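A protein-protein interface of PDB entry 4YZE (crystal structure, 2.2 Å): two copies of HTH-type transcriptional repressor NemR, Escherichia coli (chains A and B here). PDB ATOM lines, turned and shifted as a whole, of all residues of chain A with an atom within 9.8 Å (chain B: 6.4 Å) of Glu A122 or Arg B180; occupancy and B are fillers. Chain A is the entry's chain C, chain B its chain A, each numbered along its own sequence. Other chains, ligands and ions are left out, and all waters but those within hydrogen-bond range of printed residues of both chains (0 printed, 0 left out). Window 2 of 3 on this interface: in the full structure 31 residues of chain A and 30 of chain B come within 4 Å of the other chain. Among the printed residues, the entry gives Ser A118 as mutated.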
ATOM      1  N   GLU A  55     -11.869 -19.294  10.995  1.00  0.00           N
ATOM      2  CA  GLU A  55     -12.118 -18.859   9.619  1.00  0.00           C
ATOM      3  C   GLU A  55     -11.532 -17.479   9.389  1.00  0.00           C
ATOM      4  O   GLU A  55     -10.836 -17.253   8.388  1.00  0.00           O
ATOM      5  CB  GLU A  55     -13.617 -18.852   9.306  1.00  0.00           C
ATOM      6  CG  GLU A  55     -13.951 -18.837   7.817  1.00  0.00           C
ATOM      7  CD  GLU A  55     -13.931 -17.441   7.202  1.00  0.00           C
ATOM      8  OE1 GLU A  55     -14.010 -16.441   7.955  1.00  0.00           O
ATOM      9  OE2 GLU A  55     -13.847 -17.348   5.958  1.00  0.00           O
ATOM     10  N   GLY A  58      -7.905 -17.724   9.111  1.00  0.00           N
ATOM     11  CA  GLY A  58      -7.506 -18.180   7.785  1.00  0.00           C
ATOM     12  C   GLY A  58      -7.505 -17.087   6.722  1.00  0.00           C
ATOM     13  O   GLY A  58      -6.561 -16.989   5.920  1.00  0.00           O
ATOM     14  N   VAL A  59      -8.560 -16.275   6.711  1.00  0.00           N
ATOM     15  CA  VAL A  59      -8.631 -15.136   5.803  1.00  0.00           C
ATOM     16  C   VAL A  59      -7.428 -14.209   5.987  1.00  0.00           C
ATOM     17  O   VAL A  59      -6.743 -13.866   5.017  1.00  0.00           O
ATOM     18  CB  VAL A  59      -9.926 -14.340   5.964  1.00  0.00           C
ATOM     19  CG1 VAL A  59      -9.888 -13.068   5.062  1.00  0.00           C
ATOM     20  CG2 VAL A  59     -11.127 -15.209   5.576  1.00  0.00           C
ATOM     21  N   LEU A  62      -4.119 -15.798   4.724  1.00  0.00           N
ATOM     22  CA  LEU A  62      -3.970 -15.784   3.273  1.00  0.00           C
ATOM     23  C   LEU A  62      -3.624 -14.384   2.784  1.00  0.00           C
ATOM     24  O   LEU A  62      -2.707 -14.196   1.960  1.00  0.00           O
ATOM     25  CB  LEU A  62      -5.259 -16.261   2.594  1.00  0.00           C
ATOM     26  CG  LEU A  62      -5.601 -17.733   2.823  1.00  0.00           C
ATOM     27  CD1 LEU A  62      -6.852 -18.170   2.037  1.00  0.00           C
ATOM     28  CD2 LEU A  62      -4.383 -18.593   2.486  1.00  0.00           C
ATOM     29  N   GLU A  63      -4.366 -13.404   3.285  1.00  0.00           N
ATOM     30  CA  GLU A  63      -4.123 -12.014   2.913  1.00  0.00           C
ATOM     31  C   GLU A  63      -2.686 -11.602   3.216  1.00  0.00           C
ATOM     32  O   GLU A  63      -2.025 -11.036   2.367  1.00  0.00           O
ATOM     33  CB  GLU A  63      -5.118 -11.092   3.615  1.00  0.00           C
ATOM     34  CG  GLU A  63      -6.543 -11.276   3.095  1.00  0.00           C
ATOM     35  CD  GLU A  63      -7.545 -10.361   3.772  1.00  0.00           C
ATOM     36  OE1 GLU A  63      -7.146  -9.605   4.681  1.00  0.00           O
ATOM     37  OE2 GLU A  63      -8.735 -10.400   3.392  1.00  0.00           O
ATOM     38  N   GLU A 116      -8.375 -28.616  -0.920  1.00  0.00           N
ATOM     39  CA  GLU A 116      -9.443 -28.530   0.060  1.00  0.00           C
ATOM     40  C   GLU A 116     -10.391 -27.377  -0.223  1.00  0.00           C
ATOM     41  O   GLU A 116     -11.201 -27.027   0.636  1.00  0.00           O
ATOM     42  CB  GLU A 116      -8.847 -28.399   1.468  1.00  0.00           C
ATOM     43  CG  GLU A 116      -7.869 -27.237   1.619  1.00  0.00           C
ATOM     44  CD  GLU A 116      -7.007 -27.331   2.882  1.00  0.00           C
ATOM     45  OE1 GLU A 116      -7.560 -27.319   4.000  1.00  0.00           O
ATOM     46  OE2 GLU A 116      -5.769 -27.411   2.753  1.00  0.00           O
ATOM     47  N   VAL A 117     -10.302 -26.799  -1.423  1.00  0.00           N
ATOM     48  CA  VAL A 117     -11.041 -25.570  -1.729  1.00  0.00           C
ATOM     49  C   VAL A 117     -12.547 -25.678  -1.499  1.00  0.00           C
ATOM     50  O   VAL A 117     -13.173 -24.710  -1.078  1.00  0.00           O
ATOM     51  CB  VAL A 117     -10.785 -25.046  -3.159  1.00  0.00           C
ATOM     52  CG1 VAL A 117      -9.336 -24.667  -3.336  1.00  0.00           C
ATOM     53  CG2 VAL A 117     -11.210 -26.079  -4.203  1.00  0.00           C
ATOM     54  N   SER A 118     -13.118 -26.853  -1.762  1.00  0.00           N
ATOM     55  CA  SER A 118     -14.557 -27.051  -1.607  1.00  0.00           C
ATOM     56  C   SER A 118     -14.957 -26.961  -0.144  1.00  0.00           C
ATOM     57  O   SER A 118     -16.046 -26.474   0.176  1.00  0.00           O
ATOM     58  CB  SER A 118     -15.009 -28.378  -2.233  1.00  0.00           C
ATOM     59  OG  SER A 118     -14.143 -29.444  -1.882  1.00  0.00           O
ATOM     60  N   ASP A 119     -14.064 -27.403   0.742  1.00  0.00           N
ATOM     61  CA  ASP A 119     -14.305 -27.322   2.184  1.00  0.00           C
ATOM     62  C   ASP A 119     -13.878 -25.986   2.769  1.00  0.00           C
ATOM     63  O   ASP A 119     -14.089 -25.730   3.950  1.00  0.00           O
ATOM     64  CB  ASP A 119     -13.567 -28.439   2.928  1.00  0.00           C
ATOM     65  CG  ASP A 119     -14.025 -29.817   2.508  1.00  0.00           C
ATOM     66  OD1 ASP A 119     -15.246 -30.000   2.301  1.00  0.00           O
ATOM     67  OD2 ASP A 119     -13.162 -30.714   2.382  1.00  0.00           O
ATOM     68  N   LEU A 120     -13.247 -25.149   1.953  1.00  0.00           N
ATOM     69  CA  LEU A 120     -12.849 -23.821   2.410  1.00  0.00           C
ATOM     70  C   LEU A 120     -14.027 -22.872   2.358  1.00  0.00           C
ATOM     71  O   LEU A 120     -14.907 -22.987   1.494  1.00  0.00           O
ATOM     72  CB  LEU A 120     -11.719 -23.254   1.551  1.00  0.00           C
ATOM     73  CG  LEU A 120     -10.348 -23.842   1.853  1.00  0.00           C
ATOM     74  CD1 LEU A 120      -9.327 -23.293   0.893  1.00  0.00           C
ATOM     75  CD2 LEU A 120      -9.945 -23.552   3.301  1.00  0.00           C
ATOM     76  N   SER A 121     -14.025 -21.926   3.283  1.00  0.00           N
ATOM     77  CA  SER A 121     -15.027 -20.890   3.317  1.00  0.00           C
ATOM     78  C   SER A 121     -14.935 -20.053   2.056  1.00  0.00           C
ATOM     79  O   SER A 121     -13.906 -20.057   1.355  1.00  0.00           O
ATOM     80  CB  SER A 121     -14.796 -20.006   4.541  1.00  0.00           C
ATOM     81  OG  SER A 121     -13.763 -19.065   4.297  1.00  0.00           O
ATOM     82  N   GLU A 122     -16.021 -19.351   1.752  1.00  0.00           N
ATOM     83  CA  GLU A 122     -16.064 -18.486   0.581  1.00  0.00           C
ATOM     84  C   GLU A 122     -15.035 -17.369   0.685  1.00  0.00           C
ATOM     85  O   GLU A 122     -14.340 -17.084  -0.287  1.00  0.00           O
ATOM     86  CB  GLU A 122     -17.464 -17.908   0.388  1.00  0.00           C
ATOM     87  CG  GLU A 122     -18.411 -18.842  -0.367  1.00  0.00           C
ATOM     88  CD  GLU A 122     -17.812 -19.351  -1.680  1.00  0.00           C
ATOM     89  OE1 GLU A 122     -17.063 -18.602  -2.355  1.00  0.00           O
ATOM     90  OE2 GLU A 122     -18.085 -20.515  -2.039  1.00  0.00           O
ATOM     91  N   ASP A 123     -14.923 -16.759   1.865  1.00  0.00           N
ATOM     92  CA  ASP A 123     -13.947 -15.698   2.073  1.00  0.00           C
ATOM     93  C   ASP A 123     -12.513 -16.172   1.813  1.00  0.00           C
ATOM     94  O   ASP A 123     -11.699 -15.425   1.267  1.00  0.00           O
ATOM     95  CB  ASP A 123     -14.075 -15.092   3.477  1.00  0.00           C
ATOM     96  CG  ASP A 123     -15.279 -14.180   3.611  1.00  0.00           C
ATOM     97  OD1 ASP A 123     -15.806 -13.750   2.560  1.00  0.00           O
ATOM     98  OD2 ASP A 123     -15.695 -13.888   4.758  1.00  0.00           O
ATOM     99  N   MET A 124     -12.191 -17.407   2.189  1.00  0.00           N
ATOM    100  CA  MET A 124     -10.826 -17.865   1.971  1.00  0.00           C
ATOM    101  C   MET A 124     -10.595 -18.227   0.527  1.00  0.00           C
ATOM    102  O   MET A 124      -9.497 -18.041   0.007  1.00  0.00           O
ATOM    103  CB  MET A 124     -10.450 -19.029   2.882  1.00  0.00           C
ATOM    104  CG  MET A 124     -10.204 -18.579   4.319  1.00  0.00           C
ATOM    105  SD  MET A 124      -9.780 -19.942   5.394  1.00  0.00           S
ATOM    106  CE  MET A 124      -8.136 -20.357   4.795  1.00  0.00           C
ATOM    107  N   ARG A 125     -11.626 -18.747  -0.123  1.00  0.00           N
ATOM    108  CA  ARG A 125     -11.499 -19.085  -1.531  1.00  0.00           C
ATOM    109  C   ARG A 125     -11.326 -17.806  -2.338  1.00  0.00           C
ATOM    110  O   ARG A 125     -10.537 -17.745  -3.287  1.00  0.00           O
ATOM    111  CB  ARG A 125     -12.709 -19.878  -2.016  1.00  0.00           C
ATOM    112  CG  ARG A 125     -12.531 -20.433  -3.438  1.00  0.00           C
ATOM    113  CD  ARG A 125     -13.583 -21.482  -3.720  1.00  0.00           C
ATOM    114  NE  ARG A 125     -13.260 -22.348  -4.848  1.00  0.00           N
ATOM    115  CZ  ARG A 125     -13.853 -23.518  -5.056  1.00  0.00           C
ATOM    116  NH1 ARG A 125     -14.784 -23.951  -4.208  1.00  0.00           N
ATOM    117  NH2 ARG A 125     -13.514 -24.259  -6.102  1.00  0.00           N
ATOM    118  N   SER A 126     -12.055 -16.778  -1.924  1.00  0.00           N
ATOM    119  CA  SER A 126     -11.977 -15.467  -2.546  1.00  0.00           C
ATOM    120  C   SER A 126     -10.567 -14.901  -2.345  1.00  0.00           C
ATOM    121  O   SER A 126      -9.947 -14.396  -3.281  1.00  0.00           O
ATOM    122  CB  SER A 126     -13.060 -14.548  -1.963  1.00  0.00           C
ATOM    123  OG  SER A 126     -12.849 -13.204  -2.341  1.00  0.00           O
ATOM    124  N   ALA A 127     -10.035 -15.038  -1.134  1.00  0.00           N
ATOM    125  CA  ALA A 127      -8.683 -14.558  -0.867  1.00  0.00           C
ATOM    126  C   ALA A 127      -7.632 -15.315  -1.690  1.00  0.00           C
ATOM    127  O   ALA A 127      -6.615 -14.732  -2.079  1.00  0.00           O
ATOM    128  CB  ALA A 127      -8.358 -14.603   0.632  1.00  0.00           C
ATOM    129  N   MET A 128      -7.852 -16.600  -1.964  1.00  0.00           N
ATOM    130  CA  MET A 128      -6.914 -17.303  -2.837  1.00  0.00           C
ATOM    131  C   MET A 128      -7.031 -16.789  -4.296  1.00  0.00           C
ATOM    132  O   MET A 128      -6.030 -16.652  -5.000  1.00  0.00           O
ATOM    133  CB  MET A 128      -7.130 -18.814  -2.817  1.00  0.00           C
ATOM    134  CG  MET A 128      -7.006 -19.500  -1.437  1.00  0.00           C
ATOM    135  SD  MET A 128      -7.291 -21.281  -1.624  1.00  0.00           S
ATOM    136  CE  MET A 128      -9.001 -21.303  -2.136  1.00  0.00           C
ATOM    137  N   ASP A 129      -8.249 -16.527  -4.751  1.00  0.00           N
ATOM    138  CA  ASP A 129      -8.455 -16.023  -6.113  1.00  0.00           C
ATOM    139  C   ASP A 129      -7.765 -14.681  -6.337  1.00  0.00           C
ATOM    140  O   ASP A 129      -7.063 -14.500  -7.330  1.00  0.00           O
ATOM    141  CB  ASP A 129      -9.945 -15.878  -6.425  1.00  0.00           C
ATOM    142  CG  ASP A 129     -10.650 -17.213  -6.514  1.00  0.00           C
ATOM    143  OD1 ASP A 129      -9.988 -18.209  -6.892  1.00  0.00           O
ATOM    144  OD2 ASP A 129     -11.863 -17.266  -6.212  1.00  0.00           O
ATOM    145  N   LYS A 130      -7.980 -13.747  -5.411  1.00  0.00           N
ATOM    146  CA  LYS A 130      -7.382 -12.418  -5.502  1.00  0.00           C
ATOM    147  C   LYS A 130      -5.866 -12.491  -5.483  1.00  0.00           C
ATOM    148  O   LYS A 130      -5.205 -11.771  -6.221  1.00  0.00           O
ATOM    149  CB  LYS A 130      -7.872 -11.500  -4.384  1.00  0.00           C
ATOM    150  CG  LYS A 130      -8.892 -10.493  -4.855  1.00  0.00           C
ATOM    151  N   ARG A 133      -4.857 -13.649  -8.950  1.00  0.00           N
ATOM    152  CA  ARG A 133      -5.105 -12.582  -9.906  1.00  0.00           C
ATOM    153  C   ARG A 133      -4.111 -11.434  -9.759  1.00  0.00           C
ATOM    154  O   ARG A 133      -3.685 -10.850 -10.765  1.00  0.00           O
ATOM    155  CB  ARG A 133      -6.554 -12.069  -9.816  1.00  0.00           C
ATOM    156  CG  ARG A 133      -7.573 -13.081 -10.345  1.00  0.00           C
ATOM    157  CD  ARG A 133      -8.950 -12.465 -10.563  1.00  0.00           C
ATOM    158  NE  ARG A 133     -10.017 -13.459 -10.412  1.00  0.00           N
ATOM    159  CZ  ARG A 133     -10.494 -14.221 -11.394  1.00  0.00           C
ATOM    160  NH1 ARG A 133     -10.011 -14.120 -12.629  1.00  0.00           N
ATOM    161  NH2 ARG A 133     -11.463 -15.089 -11.141  1.00  0.00           N
ATOM    162  N   PHE B  99     -14.550 -30.757 -17.589  1.00  0.00           N
ATOM    163  CA  PHE B  99     -14.210 -29.921 -16.446  1.00  0.00           C
ATOM    164  C   PHE B  99     -15.258 -30.082 -15.348  1.00  0.00           C
ATOM    165  O   PHE B  99     -14.928 -30.368 -14.191  1.00  0.00           O
ATOM    166  CB  PHE B  99     -14.090 -28.456 -16.872  1.00  0.00           C
ATOM    167  CG  PHE B  99     -13.961 -27.503 -15.722  1.00  0.00           C
ATOM    168  CD1 PHE B  99     -12.961 -27.673 -14.772  1.00  0.00           C
ATOM    169  CD2 PHE B  99     -14.839 -26.433 -15.591  1.00  0.00           C
ATOM    170  CE1 PHE B  99     -12.849 -26.796 -13.698  1.00  0.00           C
ATOM    171  CE2 PHE B  99     -14.730 -25.550 -14.528  1.00  0.00           C
ATOM    172  CZ  PHE B  99     -13.733 -25.734 -13.580  1.00  0.00           C
ATOM    173  N   ILE B 105     -18.333 -29.518 -10.449  1.00  0.00           N
ATOM    174  CA  ILE B 105     -16.967 -29.669 -10.940  1.00  0.00           C
ATOM    175  C   ILE B 105     -16.490 -31.100 -10.704  1.00  0.00           C
ATOM    176  O   ILE B 105     -16.420 -31.562  -9.562  1.00  0.00           O
ATOM    177  CB  ILE B 105     -15.979 -28.679 -10.278  1.00  0.00           C
ATOM    178  CG1 ILE B 105     -16.278 -27.240 -10.707  1.00  0.00           C
ATOM    179  CG2 ILE B 105     -14.542 -29.045 -10.634  1.00  0.00           C
ATOM    180  CD1 ILE B 105     -15.424 -26.192 -10.000  1.00  0.00           C
ATOM    181  N   GLN B 175      -5.892 -23.795 -11.502  1.00  0.00           N
ATOM    182  CA  GLN B 175      -6.436 -22.459 -11.496  1.00  0.00           C
ATOM    183  C   GLN B 175      -7.922 -22.422 -11.818  1.00  0.00           C
ATOM    184  O   GLN B 175      -8.642 -21.578 -11.289  1.00  0.00           O
ATOM    185  CB  GLN B 175      -5.686 -21.629 -12.524  1.00  0.00           C
ATOM    186  CG  GLN B 175      -5.892 -20.168 -12.357  1.00  0.00           C
ATOM    187  CD  GLN B 175      -4.870 -19.385 -13.113  1.00  0.00           C
ATOM    188  OE1 GLN B 175      -3.937 -19.950 -13.693  1.00  0.00           O
ATOM    189  NE2 GLN B 175      -5.033 -18.072 -13.124  1.00  0.00           N
ATOM    190  N   ALA B 176      -8.384 -23.291 -12.719  1.00  0.00           N
ATOM    191  CA  ALA B 176      -9.819 -23.310 -13.047  1.00  0.00           C
ATOM    192  C   ALA B 176     -10.573 -23.728 -11.784  1.00  0.00           C
ATOM    193  O   ALA B 176     -11.618 -23.185 -11.449  1.00  0.00           O
ATOM    194  CB  ALA B 176     -10.102 -24.286 -14.175  1.00  0.00           C
ATOM    195  N   LYS B 177     -10.014 -24.706 -11.081  1.00  0.00           N
ATOM    196  CA  LYS B 177     -10.672 -25.289  -9.925  1.00  0.00           C
ATOM    197  C   LYS B 177     -10.804 -24.238  -8.827  1.00  0.00           C
ATOM    198  O   LYS B 177     -11.901 -24.004  -8.296  1.00  0.00           O
ATOM    199  CB  LYS B 177      -9.839 -26.477  -9.442  1.00  0.00           C
ATOM    200  CG  LYS B 177     -10.370 -27.195  -8.244  1.00  0.00           C
ATOM    201  CD  LYS B 177      -9.428 -28.360  -7.971  1.00  0.00           C
ATOM    202  CE  LYS B 177      -9.626 -28.971  -6.608  1.00  0.00           C
ATOM    203  NZ  LYS B 177      -8.415 -29.759  -6.230  1.00  0.00           N
ATOM    204  N   ILE B 178      -9.690 -23.580  -8.524  1.00  0.00           N
ATOM    205  CA  ILE B 178      -9.665 -22.537  -7.512  1.00  0.00           C
ATOM    206  C   ILE B 178     -10.631 -21.409  -7.811  1.00  0.00           C
ATOM    207  O   ILE B 178     -11.408 -21.029  -6.944  1.00  0.00           O
ATOM    208  CB  ILE B 178      -8.257 -21.954  -7.325  1.00  0.00           C
ATOM    209  CG1 ILE B 178      -7.337 -22.985  -6.684  1.00  0.00           C
ATOM    210  CG2 ILE B 178      -8.295 -20.731  -6.428  1.00  0.00           C
ATOM    211  CD1 ILE B 178      -5.880 -22.617  -6.792  1.00  0.00           C
ATOM    212  N   SER B 179     -10.582 -20.874  -9.026  1.00  0.00           N
ATOM    213  CA  SER B 179     -11.414 -19.733  -9.368  1.00  0.00           C
ATOM    214  C   SER B 179     -12.817 -20.127  -9.793  1.00  0.00           C
ATOM    215  O   SER B 179     -13.644 -19.255 -10.029  1.00  0.00           O
ATOM    216  CB  SER B 179     -10.792 -18.949 -10.514  1.00  0.00           C
ATOM    217  OG  SER B 179     -10.762 -19.731 -11.698  1.00  0.00           O
ATOM    218  N   ARG B 180     -13.086 -21.425  -9.933  1.00  0.00           N
ATOM    219  CA  ARG B 180     -14.378 -21.858 -10.495  1.00  0.00           C
ATOM    220  C   ARG B 180     -14.698 -21.145 -11.814  1.00  0.00           C
ATOM    221  O   ARG B 180     -15.809 -20.673 -12.035  1.00  0.00           O
ATOM    222  CB  ARG B 180     -15.521 -21.626  -9.501  1.00  0.00           C
ATOM    223  CG  ARG B 180     -15.257 -22.175  -8.081  1.00  0.00           C
ATOM    224  CD  ARG B 180     -16.597 -22.498  -7.432  1.00  0.00           C
ATOM    225  NE  ARG B 180     -16.648 -22.193  -6.010  1.00  0.00           N
ATOM    226  CZ  ARG B 180     -16.979 -21.005  -5.513  1.00  0.00           C
ATOM    227  NH1 ARG B 180     -17.270 -20.000  -6.324  1.00  0.00           N
ATOM    228  NH2 ARG B 180     -17.008 -20.816  -4.206  1.00  0.00           N
ATOM    229  N   SER B 181     -13.719 -21.052 -12.695  1.00  0.00           N
ATOM    230  CA  SER B 181     -13.972 -20.468 -14.008  1.00  0.00           C
ATOM    231  C   SER B 181     -13.276 -21.407 -14.949  1.00  0.00           C
ATOM    232  O   SER B 181     -12.221 -21.975 -14.592  1.00  0.00           O
ATOM    233  CB  SER B 181     -13.357 -19.066 -14.103  1.00  0.00           C
ATOM    234  OG  SER B 181     -13.424 -18.548 -15.427  1.00  0.00           O
ATOM    235  N   PHE B 182     -13.835 -21.611 -16.137  1.00  0.00           N
ATOM    236  CA  PHE B 182     -13.095 -22.387 -17.134  1.00  0.00           C
ATOM    237  C   PHE B 182     -12.229 -21.482 -18.022  1.00  0.00           C
ATOM    238  O   PHE B 182     -11.588 -21.942 -18.973  1.00  0.00           O
ATOM    239  CB  PHE B 182     -14.014 -23.311 -17.945  1.00  0.00           C
ATOM    240  CG  PHE B 182     -15.267 -22.648 -18.409  1.00  0.00           C
ATOM    241  CD1 PHE B 182     -15.253 -21.823 -19.525  1.00  0.00           C
ATOM    242  CD2 PHE B 182     -16.467 -22.845 -17.731  1.00  0.00           C
ATOM    243  CE1 PHE B 182     -16.419 -21.192 -19.957  1.00  0.00           C
ATOM    244  CE2 PHE B 182     -17.638 -22.220 -18.155  1.00  0.00           C
ATOM    245  CZ  PHE B 182     -17.611 -21.392 -19.270  1.00  0.00           C
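Of chain B, only Arg B180 (2.4 Å) comes within 4 Å of Glu A122. Of the printed residues of chain B, Arg A125 touches Lys B177, Ile B178 and Arg B180. Of the printed residues of chain B, Arg A133 touches Ser B179 (3.97 Å). Ile B105 touches none of the printed residues of chain A. Printed residues of chain A within 4 Å of Lys B177: Arg A125. Printed residues of chain A within 4 Å of Ile B178: Arg A125 and Asp A129. Of chain A, only Asp A129 (3.2 Å) and Arg A133 (3.97 Å) come within 4 Å of Ser B179. No residue of chain A comes within 4 Å of Ser B181. The nearest printed residue of chain B that does not touch Asp A129 is Arg B180 (5.4 Å).
Ser B179 touches Arg A133 (CB to NH2, 3.97 Å).
O of Ile B178 lies close to OD1 of Asp A129. The backbone carbonyl oxygen (O) of Ile B178 is in hydrogen-bond range of the guanidinium group (NE) of Arg A125, 3.1 Å away. OE2 of Glu A122 lies within salt-bridge range of NH2 of Arg B180. NH2 of Arg A125 is in hydrogen-bond range of O of Lys B177 (2.7 Å). The guanidinium group (NH1) of Arg A125 lies close to the guanidinium group (NE) of Arg B180, 3.1 Å away. The side-chain carboxylate (OD1) of Asp A129 lies close to the backbone NH (N) of Ser B179 (3.5 Å).
Of the 10 printed residues of chain B, 4 touch a printed residue of chain A.
No position is printed for both chains.
The side-chain hydroxyl of Ser B179 lies close to the backbone NH of Ser B181, 3.4 Å away. O of Gln B175 is in hydrogen-bond range of OG of Ser B179 (2.8 Å).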
